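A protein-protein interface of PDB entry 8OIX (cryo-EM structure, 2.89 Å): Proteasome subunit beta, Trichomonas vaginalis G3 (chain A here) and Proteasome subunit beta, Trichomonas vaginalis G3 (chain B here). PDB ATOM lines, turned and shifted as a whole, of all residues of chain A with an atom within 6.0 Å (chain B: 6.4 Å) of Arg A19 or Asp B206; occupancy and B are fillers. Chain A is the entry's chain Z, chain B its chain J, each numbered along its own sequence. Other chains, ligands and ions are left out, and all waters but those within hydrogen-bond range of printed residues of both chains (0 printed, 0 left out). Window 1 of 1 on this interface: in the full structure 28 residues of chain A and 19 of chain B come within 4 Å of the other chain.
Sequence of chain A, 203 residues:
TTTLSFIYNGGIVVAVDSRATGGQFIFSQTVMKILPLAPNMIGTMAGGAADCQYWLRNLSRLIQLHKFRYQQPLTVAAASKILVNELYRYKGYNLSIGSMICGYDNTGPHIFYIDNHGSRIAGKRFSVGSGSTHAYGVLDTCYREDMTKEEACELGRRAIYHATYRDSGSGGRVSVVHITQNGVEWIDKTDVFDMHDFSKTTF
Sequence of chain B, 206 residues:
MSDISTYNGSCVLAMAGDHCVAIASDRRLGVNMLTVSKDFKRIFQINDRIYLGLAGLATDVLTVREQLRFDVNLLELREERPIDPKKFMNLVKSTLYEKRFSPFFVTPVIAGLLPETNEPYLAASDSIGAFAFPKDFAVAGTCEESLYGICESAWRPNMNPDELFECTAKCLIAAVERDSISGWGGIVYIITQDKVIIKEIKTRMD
The side-chain hydroxyl (OG1) of Thr B35 lies within hydrogen-bond range of the backbone carbonyl oxygen (O) of Tyr A165. OG of Ser B180 sits close to OG1 of Thr A21, 3.4 Å away. O of Tyr A165 is in hydrogen-bond range of NE1 of Trp B184 (2.6 Å). NE of Arg B204 lies close to NE2 of Gln A29, 3.4 Å away. The guanidinium group (NH2) of Arg B204 is in hydrogen-bond range of the backbone carbonyl oxygen (O) of Gly A172 (2.8 Å). The side-chain carboxylate of Asp A191 lies within salt-bridge range of the guanidinium group of Arg B204, 2.4 Å away. The chain-end carboxylate (OXT) of Asp B206 lies within salt-bridge range of the guanidinium group (NH1) of Arg A19, at 2.4 Å. The side-chain amide nitrogen of Gln A29 is in hydrogen-bond range of the side-chain carboxylate of Asp B206, at 3.0 Å. The side-chain carboxylate (OD2) of Asp B206 is in hydrogen-bond range of the backbone NH (N) of Gly A172, 2.7 Å away. OXT of Asp B206 lies close to O of Thr A164 (3.2 Å). O of Asp A167 lies close to OXT of Asp B206, 3.5 Å away. O of Ser A170 lies close to OXT of Asp B206, at 3.0 Å.
The backbone carbonyl oxygen of Met B205 sits at hydrogen-bond distance from the indole nitrogen of Trp B184, at 3.3 Å. The side-chain carboxylate (OD2) of Asp A17 is in hydrogen-bond range of the backbone NH (N) of Arg A19, 2.8 Å away. The backbone carbonyl oxygen (O) of Arg A19 is in hydrogen-bond range of the side-chain amino group (NZ) of Lys A33. The guanidinium group (NH1) of Arg A19 is in hydrogen-bond range of the backbone carbonyl oxygen (O) of Ser A168 (2.7 Å). The backbone NH (N) of Arg A19 lies within hydrogen-bond range of the backbone carbonyl oxygen (O) of Gly A171 (3.1 Å). The backbone NH (N) of Phe A193 is in hydrogen-bond range of the side-chain carboxylate (OD1) of Asp A191, 3.0 Å away.
NH1 of Arg A19 touches CA of Ser B180, at 3.9 Å. CD1 of Ile A26 touches O of Glu B177, at 3.1 Å. Thr A164 touches Trp B184 (O to CZ2, 3.7 Å). Tyr A165 touches Met B205. Ser B180 touches Ser A168. Ser A168 touches Ile B181 (OG to CG2, 3.6 Å). CA of Gly A171 touches OD2 of Asp B206, 3.2 Å away. Val A192 touches Asp B206. Phe A193 touches Thr B203 (CE1 to O, 3.2 Å). Phe A193 touches Arg B204.
Arg A19 touches two residues of chain B. Printed residues of chain B within 4 Å of Thr A21: Ser B180 (3.4 Å). Printed residues of chain B within 4 Å of Gly A172: Arg B204 (2.8 Å) and Asp B206 (2.7 Å). Printed residues of chain B within 4 Å of Asp A191: Arg B204. Of the printed residues of chain A, Asp B179 touches Ile A26. Of the printed residues of chain B, Tyr A165 touches Thr B35, Trp B184 and Met B205. Asp A17 touches none of the printed residues of chain B. Lys A33 touches none of the printed residues of chain B. The nearest residue of chain A that does not touch Asp B206 is Ser A168 (4.04 Å).
Of the 25 printed residues of chain A, 14 touch a printed residue of chain B. Hydrophobic or aromatic side chains of chain B within 4 Å of the printed part of chain A: Ile B181, Trp B184 and Met B205. Among the printed residues, 25 pairs touch across the chains. Among the printed residues, Asp or Glu carboxylates within 4 Å of a Lys or Arg side-chain nitrogen of the other chain: Arg A19 with Asp B206 (3.0 Å) and Asp A191 with Arg B204 (2.4 Å).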
ATOM      1  N   THR A   1      -9.665 -14.803  19.217  1.00  0.00           N
ATOM      2  CA  THR A   1      -9.773 -15.849  18.211  1.00  0.00           C
ATOM      3  C   THR A   1     -10.777 -15.404  17.148  1.00  0.00           C
ATOM      4  O   THR A   1     -11.663 -14.601  17.434  1.00  0.00           O
ATOM      5  CB  THR A   1     -10.214 -17.189  18.860  1.00  0.00           C
ATOM      6  OG1 THR A   1      -9.190 -17.650  19.748  1.00  0.00           O
ATOM      7  CG2 THR A   1     -10.467 -18.265  17.818  1.00  0.00           C
ATOM      8  N   ASP A  17      -7.879 -17.432  11.944  1.00  0.00           N
ATOM      9  CA  ASP A  17      -6.671 -16.765  12.398  1.00  0.00           C
ATOM     10  C   ASP A  17      -5.768 -17.775  13.105  1.00  0.00           C
ATOM     11  O   ASP A  17      -6.070 -18.967  13.198  1.00  0.00           O
ATOM     12  CB  ASP A  17      -7.013 -15.593  13.316  1.00  0.00           C
ATOM     13  CG  ASP A  17      -7.383 -16.033  14.716  1.00  0.00           C
ATOM     14  OD1 ASP A  17      -8.520 -16.494  14.925  1.00  0.00           O
ATOM     15  OD2 ASP A  17      -6.531 -15.905  15.619  1.00  0.00           O
ATOM     16  N   SER A  18      -4.638 -17.294  13.622  1.00  0.00           N
ATOM     17  CA  SER A  18      -3.687 -18.175  14.285  1.00  0.00           C
ATOM     18  C   SER A  18      -3.212 -17.613  15.618  1.00  0.00           C
ATOM     19  O   SER A  18      -2.198 -18.071  16.151  1.00  0.00           O
ATOM     20  CB  SER A  18      -2.488 -18.453  13.376  1.00  0.00           C
ATOM     21  OG  SER A  18      -2.862 -19.262  12.274  1.00  0.00           O
ATOM     22  N   ARG A  19      -3.925 -16.641  16.175  1.00  0.00           N
ATOM     23  CA  ARG A  19      -3.498 -15.984  17.401  1.00  0.00           C
ATOM     24  C   ARG A  19      -4.104 -16.663  18.620  1.00  0.00           C
ATOM     25  O   ARG A  19      -5.324 -16.840  18.703  1.00  0.00           O
ATOM     26  CB  ARG A  19      -3.892 -14.510  17.383  1.00  0.00           C
ATOM     27  CG  ARG A  19      -3.686 -13.808  18.707  1.00  0.00           C
ATOM     28  CD  ARG A  19      -3.830 -12.318  18.544  1.00  0.00           C
ATOM     29  NE  ARG A  19      -2.803 -11.777  17.665  1.00  0.00           N
ATOM     30  CZ  ARG A  19      -2.638 -10.487  17.412  1.00  0.00           C
ATOM     31  NH1 ARG A  19      -3.424  -9.572  17.955  1.00  0.00           N
ATOM     32  NH2 ARG A  19      -1.659 -10.106  16.599  1.00  0.00           N
ATOM     33  N   ALA A  20      -3.248 -17.039  19.564  1.00  0.00           N
ATOM     34  CA  ALA A  20      -3.654 -17.398  20.915  1.00  0.00           C
ATOM     35  C   ALA A  20      -3.153 -16.309  21.849  1.00  0.00           C
ATOM     36  O   ALA A  20      -1.943 -16.076  21.934  1.00  0.00           O
ATOM     37  CB  ALA A  20      -3.099 -18.760  21.327  1.00  0.00           C
ATOM     38  N   THR A  21      -4.078 -15.639  22.532  1.00  0.00           N
ATOM     39  CA  THR A  21      -3.737 -14.530  23.410  1.00  0.00           C
ATOM     40  C   THR A  21      -4.630 -14.551  24.641  1.00  0.00           C
ATOM     41  O   THR A  21      -5.851 -14.699  24.528  1.00  0.00           O
ATOM     42  CB  THR A  21      -3.858 -13.185  22.679  1.00  0.00           C
ATOM     43  OG1 THR A  21      -3.671 -12.112  23.611  1.00  0.00           O
ATOM     44  CG2 THR A  21      -5.213 -13.045  22.009  1.00  0.00           C
ATOM     45  N   ILE A  26       0.248 -11.859  23.512  1.00  0.00           N
ATOM     46  CA  ILE A  26      -0.009 -12.777  22.407  1.00  0.00           C
ATOM     47  C   ILE A  26       0.859 -14.007  22.643  1.00  0.00           C
ATOM     48  O   ILE A  26       2.059 -13.999  22.370  1.00  0.00           O
ATOM     49  CB  ILE A  26       0.285 -12.135  21.052  1.00  0.00           C
ATOM     50  CG1 ILE A  26      -0.668 -10.974  20.790  1.00  0.00           C
ATOM     51  CG2 ILE A  26       0.160 -13.163  19.943  1.00  0.00           C
ATOM     52  CD1 ILE A  26      -0.206 -10.060  19.688  1.00  0.00           C
ATOM     53  N   SER A  28       0.748 -16.839  21.080  1.00  0.00           N
ATOM     54  CA  SER A  28       1.208 -17.391  19.814  1.00  0.00           C
ATOM     55  C   SER A  28       0.507 -16.698  18.656  1.00  0.00           C
ATOM     56  O   SER A  28      -0.599 -16.176  18.806  1.00  0.00           O
ATOM     57  CB  SER A  28       0.971 -18.902  19.745  1.00  0.00           C
ATOM     58  OG  SER A  28       1.560 -19.451  18.582  1.00  0.00           O
ATOM     59  N   GLN A  29       1.174 -16.697  17.501  1.00  0.00           N
ATOM     60  CA  GLN A  29       0.580 -16.256  16.244  1.00  0.00           C
ATOM     61  C   GLN A  29       0.563 -17.360  15.194  1.00  0.00           C
ATOM     62  O   GLN A  29       0.237 -17.088  14.034  1.00  0.00           O
ATOM     63  CB  GLN A  29       1.321 -15.036  15.690  1.00  0.00           C
ATOM     64  CG  GLN A  29       1.155 -13.770  16.505  1.00  0.00           C
ATOM     65  CD  GLN A  29      -0.041 -12.955  16.073  1.00  0.00           C
ATOM     66  OE1 GLN A  29      -1.134 -13.102  16.615  1.00  0.00           O
ATOM     67  NE2 GLN A  29       0.162 -12.083  15.095  1.00  0.00           N
ATOM     68  N   THR A  30       0.926 -18.590  15.561  1.00  0.00           N
ATOM     69  CA  THR A  30       0.962 -19.711  14.630  1.00  0.00           C
ATOM     70  C   THR A  30       0.088 -20.866  15.109  1.00  0.00           C
ATOM     71  O   THR A  30       0.359 -22.029  14.807  1.00  0.00           O
ATOM     72  CB  THR A  30       2.399 -20.186  14.411  1.00  0.00           C
ATOM     73  OG1 THR A  30       3.014 -20.461  15.675  1.00  0.00           O
ATOM     74  CG2 THR A  30       3.203 -19.122  13.680  1.00  0.00           C
ATOM     75  N   VAL A  31      -0.966 -20.553  15.861  1.00  0.00           N
ATOM     76  CA  VAL A  31      -1.884 -21.577  16.343  1.00  0.00           C
ATOM     77  C   VAL A  31      -2.738 -22.092  15.193  1.00  0.00           C
ATOM     78  O   VAL A  31      -3.340 -21.313  14.446  1.00  0.00           O
ATOM     79  CB  VAL A  31      -2.755 -21.016  17.475  1.00  0.00           C
ATOM     80  CG1 VAL A  31      -3.880 -21.968  17.790  1.00  0.00           C
ATOM     81  CG2 VAL A  31      -1.908 -20.782  18.704  1.00  0.00           C
ATOM     82  N   LYS A  33      -5.993 -23.460  14.078  1.00  0.00           N
ATOM     83  CA  LYS A  33      -7.359 -23.464  14.579  1.00  0.00           C
ATOM     84  C   LYS A  33      -8.291 -24.312  13.725  1.00  0.00           C
ATOM     85  O   LYS A  33      -9.507 -24.274  13.929  1.00  0.00           O
ATOM     86  CB  LYS A  33      -7.889 -22.034  14.677  1.00  0.00           C
ATOM     87  CG  LYS A  33      -7.101 -21.147  15.624  1.00  0.00           C
ATOM     88  CD  LYS A  33      -7.801 -19.822  15.843  1.00  0.00           C
ATOM     89  CE  LYS A  33      -6.989 -18.909  16.742  1.00  0.00           C
ATOM     90  NZ  LYS A  33      -6.754 -19.514  18.078  1.00  0.00           N
ATOM     91  N   TYR A 161      -8.847 -11.445   7.963  1.00  0.00           N
ATOM     92  CA  TYR A 161      -7.900 -10.339   8.055  1.00  0.00           C
ATOM     93  C   TYR A 161      -8.529  -9.122   8.723  1.00  0.00           C
ATOM     94  O   TYR A 161      -7.903  -8.480   9.574  1.00  0.00           O
ATOM     95  CB  TYR A 161      -7.382  -9.971   6.665  1.00  0.00           C
ATOM     96  CG  TYR A 161      -7.004  -8.514   6.532  1.00  0.00           C
ATOM     97  CD1 TYR A 161      -5.898  -8.000   7.195  1.00  0.00           C
ATOM     98  CD2 TYR A 161      -7.761  -7.652   5.754  1.00  0.00           C
ATOM     99  CE1 TYR A 161      -5.558  -6.669   7.083  1.00  0.00           C
ATOM    100  CE2 TYR A 161      -7.426  -6.321   5.634  1.00  0.00           C
ATOM    101  CZ  TYR A 161      -6.323  -5.834   6.301  1.00  0.00           C
ATOM    102  OH  TYR A 161      -5.985  -4.507   6.184  1.00  0.00           O
ATOM    103  N   THR A 164      -8.838  -9.798  12.368  1.00  0.00           N
ATOM    104  CA  THR A 164      -7.551  -9.649  13.038  1.00  0.00           C
ATOM    105  C   THR A 164      -7.202  -8.182  13.223  1.00  0.00           C
ATOM    106  O   THR A 164      -6.666  -7.788  14.264  1.00  0.00           O
ATOM    107  CB  THR A 164      -6.448 -10.361  12.254  1.00  0.00           C
ATOM    108  OG1 THR A 164      -6.329  -9.775  10.952  1.00  0.00           O
ATOM    109  CG2 THR A 164      -6.743 -11.845  12.131  1.00  0.00           C
ATOM    110  N   TYR A 165      -7.490  -7.362  12.215  1.00  0.00           N
ATOM    111  CA  TYR A 165      -7.219  -5.934  12.326  1.00  0.00           C
ATOM    112  C   TYR A 165      -8.050  -5.303  13.434  1.00  0.00           C
ATOM    113  O   TYR A 165      -7.524  -4.571  14.279  1.00  0.00           O
ATOM    114  CB  TYR A 165      -7.481  -5.242  10.988  1.00  0.00           C
ATOM    115  CG  TYR A 165      -7.243  -3.751  11.037  1.00  0.00           C
ATOM    116  CD1 TYR A 165      -8.247  -2.883  11.444  1.00  0.00           C
ATOM    117  CD2 TYR A 165      -6.009  -3.213  10.703  1.00  0.00           C
ATOM    118  CE1 TYR A 165      -8.035  -1.530  11.504  1.00  0.00           C
ATOM    119  CE2 TYR A 165      -5.790  -1.854  10.759  1.00  0.00           C
ATOM    120  CZ  TYR A 165      -6.808  -1.020  11.161  1.00  0.00           C
ATOM    121  OH  TYR A 165      -6.608   0.335  11.226  1.00  0.00           O
ATOM    122  N   ASP A 167      -9.794  -6.787  15.891  1.00  0.00           N
ATOM    123  CA  ASP A 167      -9.825  -7.508  17.156  1.00  0.00           C
ATOM    124  C   ASP A 167      -8.405  -7.787  17.621  1.00  0.00           C
ATOM    125  O   ASP A 167      -7.579  -8.279  16.846  1.00  0.00           O
ATOM    126  CB  ASP A 167     -10.605  -8.817  17.034  1.00  0.00           C
ATOM    127  CG  ASP A 167     -10.941  -9.420  18.377  1.00  0.00           C
ATOM    128  OD1 ASP A 167     -11.588  -8.734  19.194  1.00  0.00           O
ATOM    129  OD2 ASP A 167     -10.557 -10.583  18.615  1.00  0.00           O
ATOM    130  N   SER A 168      -8.124  -7.471  18.886  1.00  0.00           N
ATOM    131  CA  SER A 168      -6.826  -7.820  19.450  1.00  0.00           C
ATOM    132  C   SER A 168      -6.680  -9.324  19.617  1.00  0.00           C
ATOM    133  O   SER A 168      -5.562  -9.847  19.565  1.00  0.00           O
ATOM    134  CB  SER A 168      -6.633  -7.136  20.799  1.00  0.00           C
ATOM    135  OG  SER A 168      -7.572  -7.612  21.742  1.00  0.00           O
ATOM    136  N   GLY A 169      -7.790 -10.033  19.811  1.00  0.00           N
ATOM    137  CA  GLY A 169      -7.753 -11.469  20.014  1.00  0.00           C
ATOM    138  C   GLY A 169      -7.489 -12.273  18.763  1.00  0.00           C
ATOM    139  O   GLY A 169      -7.233 -13.477  18.866  1.00  0.00           O
ATOM    140  N   SER A 170      -7.544 -11.644  17.594  1.00  0.00           N
ATOM    141  CA  SER A 170      -7.347 -12.320  16.324  1.00  0.00           C
ATOM    142  C   SER A 170      -6.095 -11.780  15.652  1.00  0.00           C
ATOM    143  O   SER A 170      -5.822 -10.577  15.700  1.00  0.00           O
ATOM    144  CB  SER A 170      -8.555 -12.131  15.410  1.00  0.00           C
ATOM    145  OG  SER A 170      -9.758 -12.381  16.112  1.00  0.00           O
ATOM    146  N   GLY A 171      -5.340 -12.675  15.029  1.00  0.00           N
ATOM    147  CA  GLY A 171      -4.104 -12.276  14.390  1.00  0.00           C
ATOM    148  C   GLY A 171      -3.378 -13.483  13.845  1.00  0.00           C
ATOM    149  O   GLY A 171      -3.921 -14.587  13.787  1.00  0.00           O
ATOM    150  N   GLY A 172      -2.138 -13.255  13.442  1.00  0.00           N
ATOM    151  CA  GLY A 172      -1.295 -14.331  12.951  1.00  0.00           C
ATOM    152  C   GLY A 172      -1.463 -14.523  11.460  1.00  0.00           C
ATOM    153  O   GLY A 172      -1.302 -13.584  10.689  1.00  0.00           O
ATOM    154  N   ARG A 173      -1.781 -15.749  11.058  1.00  0.00           N
ATOM    155  CA  ARG A 173      -1.957 -16.085   9.654  1.00  0.00           C
ATOM    156  C   ARG A 173      -3.300 -16.765   9.437  1.00  0.00           C
ATOM    157  O   ARG A 173      -3.727 -17.594  10.244  1.00  0.00           O
ATOM    158  CB  ARG A 173      -0.816 -16.980   9.161  1.00  0.00           C
ATOM    159  CG  ARG A 173      -0.535 -18.176  10.049  1.00  0.00           C
ATOM    160  CD  ARG A 173       0.770 -18.839   9.660  1.00  0.00           C
ATOM    161  NE  ARG A 173       1.109 -19.946  10.544  1.00  0.00           N
ATOM    162  CZ  ARG A 173       2.190 -20.702  10.415  1.00  0.00           C
ATOM    163  NH1 ARG A 173       3.065 -20.495   9.445  1.00  0.00           N
ATOM    164  NH2 ARG A 173       2.400 -21.689  11.281  1.00  0.00           N
ATOM    165  N   ASP A 191      -0.168 -14.695   5.870  1.00  0.00           N
ATOM    166  CA  ASP A 191       0.089 -13.722   6.924  1.00  0.00           C
ATOM    167  C   ASP A 191      -0.779 -12.485   6.724  1.00  0.00           C
ATOM    168  O   ASP A 191      -0.710 -11.832   5.678  1.00  0.00           O
ATOM    169  CB  ASP A 191       1.570 -13.348   6.932  1.00  0.00           C
ATOM    170  CG  ASP A 191       1.938 -12.423   8.076  1.00  0.00           C
ATOM    171  OD1 ASP A 191       1.073 -12.146   8.932  1.00  0.00           O
ATOM    172  OD2 ASP A 191       3.101 -11.972   8.120  1.00  0.00           O
ATOM    173  N   VAL A 192      -1.604 -12.169   7.728  1.00  0.00           N
ATOM    174  CA  VAL A 192      -2.466 -10.993   7.655  1.00  0.00           C
ATOM    175  C   VAL A 192      -1.649  -9.717   7.547  1.00  0.00           C
ATOM    176  O   VAL A 192      -2.166  -8.686   7.105  1.00  0.00           O
ATOM    177  CB  VAL A 192      -3.403 -10.914   8.878  1.00  0.00           C
ATOM    178  CG1 VAL A 192      -4.294 -12.129   8.951  1.00  0.00           C
ATOM    179  CG2 VAL A 192      -2.607 -10.751  10.154  1.00  0.00           C
ATOM    180  N   PHE A 193      -0.380  -9.758   7.957  1.00  0.00           N
ATOM    181  CA  PHE A 193       0.497  -8.609   7.781  1.00  0.00           C
ATOM    182  C   PHE A 193       0.680  -8.293   6.303  1.00  0.00           C
ATOM    183  O   PHE A 193       0.750  -7.121   5.911  1.00  0.00           O
ATOM    184  CB  PHE A 193       1.844  -8.888   8.448  1.00  0.00           C
ATOM    185  CG  PHE A 193       2.720  -7.682   8.591  1.00  0.00           C
ATOM    186  CD1 PHE A 193       2.180  -6.409   8.604  1.00  0.00           C
ATOM    187  CD2 PHE A 193       4.088  -7.824   8.718  1.00  0.00           C
ATOM    188  CE1 PHE A 193       2.993  -5.304   8.739  1.00  0.00           C
ATOM    189  CE2 PHE A 193       4.903  -6.723   8.851  1.00  0.00           C
ATOM    190  CZ  PHE A 193       4.356  -5.462   8.863  1.00  0.00           C
ATOM    191  N   THR B  35     -10.058  -2.628  17.964  1.00  0.00           N
ATOM    192  CA  THR B  35      -9.275  -1.548  17.379  1.00  0.00           C
ATOM    193  C   THR B  35     -10.219  -0.460  16.885  1.00  0.00           C
ATOM    194  O   THR B  35     -11.041  -0.701  15.994  1.00  0.00           O
ATOM    195  CB  THR B  35      -8.411  -2.065  16.232  1.00  0.00           C
ATOM    196  OG1 THR B  35      -7.637  -3.182  16.683  1.00  0.00           O
ATOM    197  CG2 THR B  35      -7.476  -0.973  15.739  1.00  0.00           C
ATOM    198  N   VAL B 176       5.206  -4.845  20.495  1.00  0.00           N
ATOM    199  CA  VAL B 176       3.804  -4.700  20.108  1.00  0.00           C
ATOM    200  C   VAL B 176       3.266  -5.996  19.513  1.00  0.00           C
ATOM    201  O   VAL B 176       2.093  -6.334  19.698  1.00  0.00           O
ATOM    202  CB  VAL B 176       3.612  -3.511  19.145  1.00  0.00           C
ATOM    203  CG1 VAL B 176       4.034  -2.212  19.803  1.00  0.00           C
ATOM    204  CG2 VAL B 176       4.361  -3.725  17.843  1.00  0.00           C
ATOM    205  N   GLU B 177       4.101  -6.738  18.783  1.00  0.00           N
ATOM    206  CA  GLU B 177       3.639  -7.974  18.169  1.00  0.00           C
ATOM    207  C   GLU B 177       3.387  -9.085  19.177  1.00  0.00           C
ATOM    208  O   GLU B 177       2.810 -10.112  18.806  1.00  0.00           O
ATOM    209  CB  GLU B 177       4.645  -8.439  17.121  1.00  0.00           C
ATOM    210  CG  GLU B 177       4.681  -7.563  15.890  1.00  0.00           C
ATOM    211  CD  GLU B 177       5.774  -7.967  14.934  1.00  0.00           C
ATOM    212  OE1 GLU B 177       6.592  -8.834  15.303  1.00  0.00           O
ATOM    213  OE2 GLU B 177       5.811  -7.424  13.811  1.00  0.00           O
ATOM    214  N   ASP B 179       1.926  -8.041  22.162  1.00  0.00           N
ATOM    215  CA  ASP B 179       0.809  -7.449  22.885  1.00  0.00           C
ATOM    216  C   ASP B 179      -0.391  -7.395  21.951  1.00  0.00           C
ATOM    217  O   ASP B 179      -0.326  -6.773  20.886  1.00  0.00           O
ATOM    218  CB  ASP B 179       1.171  -6.054  23.396  1.00  0.00           C
ATOM    219  CG  ASP B 179       0.120  -5.484  24.325  1.00  0.00           C
ATOM    220  OD1 ASP B 179      -0.815  -6.222  24.693  1.00  0.00           O
ATOM    221  OD2 ASP B 179       0.239  -4.301  24.704  1.00  0.00           O
ATOM    222  N   SER B 180      -1.484  -8.048  22.349  1.00  0.00           N
ATOM    223  CA  SER B 180      -2.651  -8.114  21.478  1.00  0.00           C
ATOM    224  C   SER B 180      -3.299  -6.748  21.314  1.00  0.00           C
ATOM    225  O   SER B 180      -3.729  -6.388  20.212  1.00  0.00           O
ATOM    226  CB  SER B 180      -3.658  -9.125  22.024  1.00  0.00           C
ATOM    227  OG  SER B 180      -4.106  -8.750  23.314  1.00  0.00           O
ATOM    228  N   ILE B 181      -3.340  -5.960  22.383  1.00  0.00           N
ATOM    229  CA  ILE B 181      -4.091  -4.712  22.385  1.00  0.00           C
ATOM    230  C   ILE B 181      -3.197  -3.559  21.955  1.00  0.00           C
ATOM    231  O   ILE B 181      -3.605  -2.392  22.000  1.00  0.00           O
ATOM    232  CB  ILE B 181      -4.709  -4.448  23.767  1.00  0.00           C
ATOM    233  CG1 ILE B 181      -3.625  -4.454  24.840  1.00  0.00           C
ATOM    234  CG2 ILE B 181      -5.760  -5.496  24.085  1.00  0.00           C
ATOM    235  CD1 ILE B 181      -4.132  -4.049  26.189  1.00  0.00           C
ATOM    236  N   SER B 182      -1.976  -3.871  21.533  1.00  0.00           N
ATOM    237  CA  SER B 182      -1.031  -2.866  21.076  1.00  0.00           C
ATOM    238  C   SER B 182      -0.507  -3.220  19.694  1.00  0.00           C
ATOM    239  O   SER B 182      -0.490  -4.388  19.294  1.00  0.00           O
ATOM    240  CB  SER B 182       0.144  -2.716  22.033  1.00  0.00           C
ATOM    241  OG  SER B 182       1.151  -1.920  21.442  1.00  0.00           O
ATOM    242  N   GLY B 183      -0.078  -2.192  18.970  1.00  0.00           N
ATOM    243  CA  GLY B 183       0.464  -2.353  17.638  1.00  0.00           C
ATOM    244  C   GLY B 183      -0.192  -1.421  16.645  1.00  0.00           C
ATOM    245  O   GLY B 183      -0.271  -0.213  16.889  1.00  0.00           O
ATOM    246  N   TRP B 184      -0.693  -1.975  15.545  1.00  0.00           N
ATOM    247  CA  TRP B 184      -1.320  -1.210  14.470  1.00  0.00           C
ATOM    248  C   TRP B 184      -0.489   0.017  14.099  1.00  0.00           C
ATOM    249  O   TRP B 184      -0.954   1.157  14.119  1.00  0.00           O
ATOM    250  CB  TRP B 184      -2.744  -0.827  14.857  1.00  0.00           C
ATOM    251  CG  TRP B 184      -3.671  -2.000  14.863  1.00  0.00           C
ATOM    252  CD1 TRP B 184      -4.486  -2.402  13.849  1.00  0.00           C
ATOM    253  CD2 TRP B 184      -3.818  -2.970  15.905  1.00  0.00           C
ATOM    254  NE1 TRP B 184      -5.168  -3.537  14.212  1.00  0.00           N
ATOM    255  CE2 TRP B 184      -4.771  -3.909  15.469  1.00  0.00           C
ATOM    256  CE3 TRP B 184      -3.248  -3.127  17.171  1.00  0.00           C
ATOM    257  CZ2 TRP B 184      -5.169  -4.986  16.255  1.00  0.00           C
ATOM    258  CZ3 TRP B 184      -3.647  -4.195  17.948  1.00  0.00           C
ATOM    259  CH2 TRP B 184      -4.596  -5.112  17.488  1.00  0.00           C
ATOM    260  N   THR B 203       4.326  -1.889  11.775  1.00  0.00           N
ATOM    261  CA  THR B 203       4.151  -3.035  12.651  1.00  0.00           C
ATOM    262  C   THR B 203       2.991  -3.875  12.137  1.00  0.00           C
ATOM    263  O   THR B 203       2.268  -3.484  11.218  1.00  0.00           O
ATOM    264  CB  THR B 203       3.894  -2.601  14.100  1.00  0.00           C
ATOM    265  OG1 THR B 203       2.550  -2.122  14.226  1.00  0.00           O
ATOM    266  CG2 THR B 203       4.854  -1.499  14.507  1.00  0.00           C
ATOM    267  N   ARG B 204       2.824  -5.048  12.737  1.00  0.00           N
ATOM    268  CA  ARG B 204       1.683  -5.886  12.400  1.00  0.00           C
ATOM    269  C   ARG B 204       0.379  -5.175  12.731  1.00  0.00           C
ATOM    270  O   ARG B 204       0.255  -4.510  13.763  1.00  0.00           O
ATOM    271  CB  ARG B 204       1.755  -7.218  13.141  1.00  0.00           C
ATOM    272  CG  ARG B 204       2.901  -8.099  12.712  1.00  0.00           C
ATOM    273  CD  ARG B 204       2.740  -9.486  13.287  1.00  0.00           C
ATOM    274  NE  ARG B 204       1.575 -10.155  12.725  1.00  0.00           N
ATOM    275  CZ  ARG B 204       1.588 -10.862  11.605  1.00  0.00           C
ATOM    276  NH1 ARG B 204       2.699 -11.026  10.906  1.00  0.00           N
ATOM    277  NH2 ARG B 204       0.461 -11.418  11.174  1.00  0.00           N
ATOM    278  N   MET B 205      -0.598  -5.324  11.842  1.00  0.00           N
ATOM    279  CA  MET B 205      -1.903  -4.685  11.972  1.00  0.00           C
ATOM    280  C   MET B 205      -2.949  -5.682  12.444  1.00  0.00           C
ATOM    281  O   MET B 205      -4.090  -5.671  11.981  1.00  0.00           O
ATOM    282  CB  MET B 205      -2.318  -4.057  10.647  1.00  0.00           C
ATOM    283  CG  MET B 205      -1.394  -2.958  10.160  1.00  0.00           C
ATOM    284  SD  MET B 205      -1.678  -1.398  11.008  1.00  0.00           S
ATOM    285  CE  MET B 205      -0.243  -0.463  10.495  1.00  0.00           C
ATOM    286  N   ASP B 206      -2.568  -6.562  13.362  1.00  0.00           N
ATOM    287  CA  ASP B 206      -3.495  -7.514  13.954  1.00  0.00           C
ATOM    288  C   ASP B 206      -3.335  -7.586  15.469  1.00  0.00           C
ATOM    289  O   ASP B 206      -2.363  -7.082  16.030  1.00  0.00           O
ATOM    290  CB  ASP B 206      -3.294  -8.899  13.335  1.00  0.00           C
ATOM    291  CG  ASP B 206      -1.888  -9.432  13.533  1.00  0.00           C
ATOM    292  OD1 ASP B 206      -1.022  -8.678  14.018  1.00  0.00           O
ATOM    293  OD2 ASP B 206      -1.648 -10.611  13.204  1.00  0.00           O
ATOM    294  OXT ASP B 206      -4.179  -8.147  16.168  1.00  0.00           O
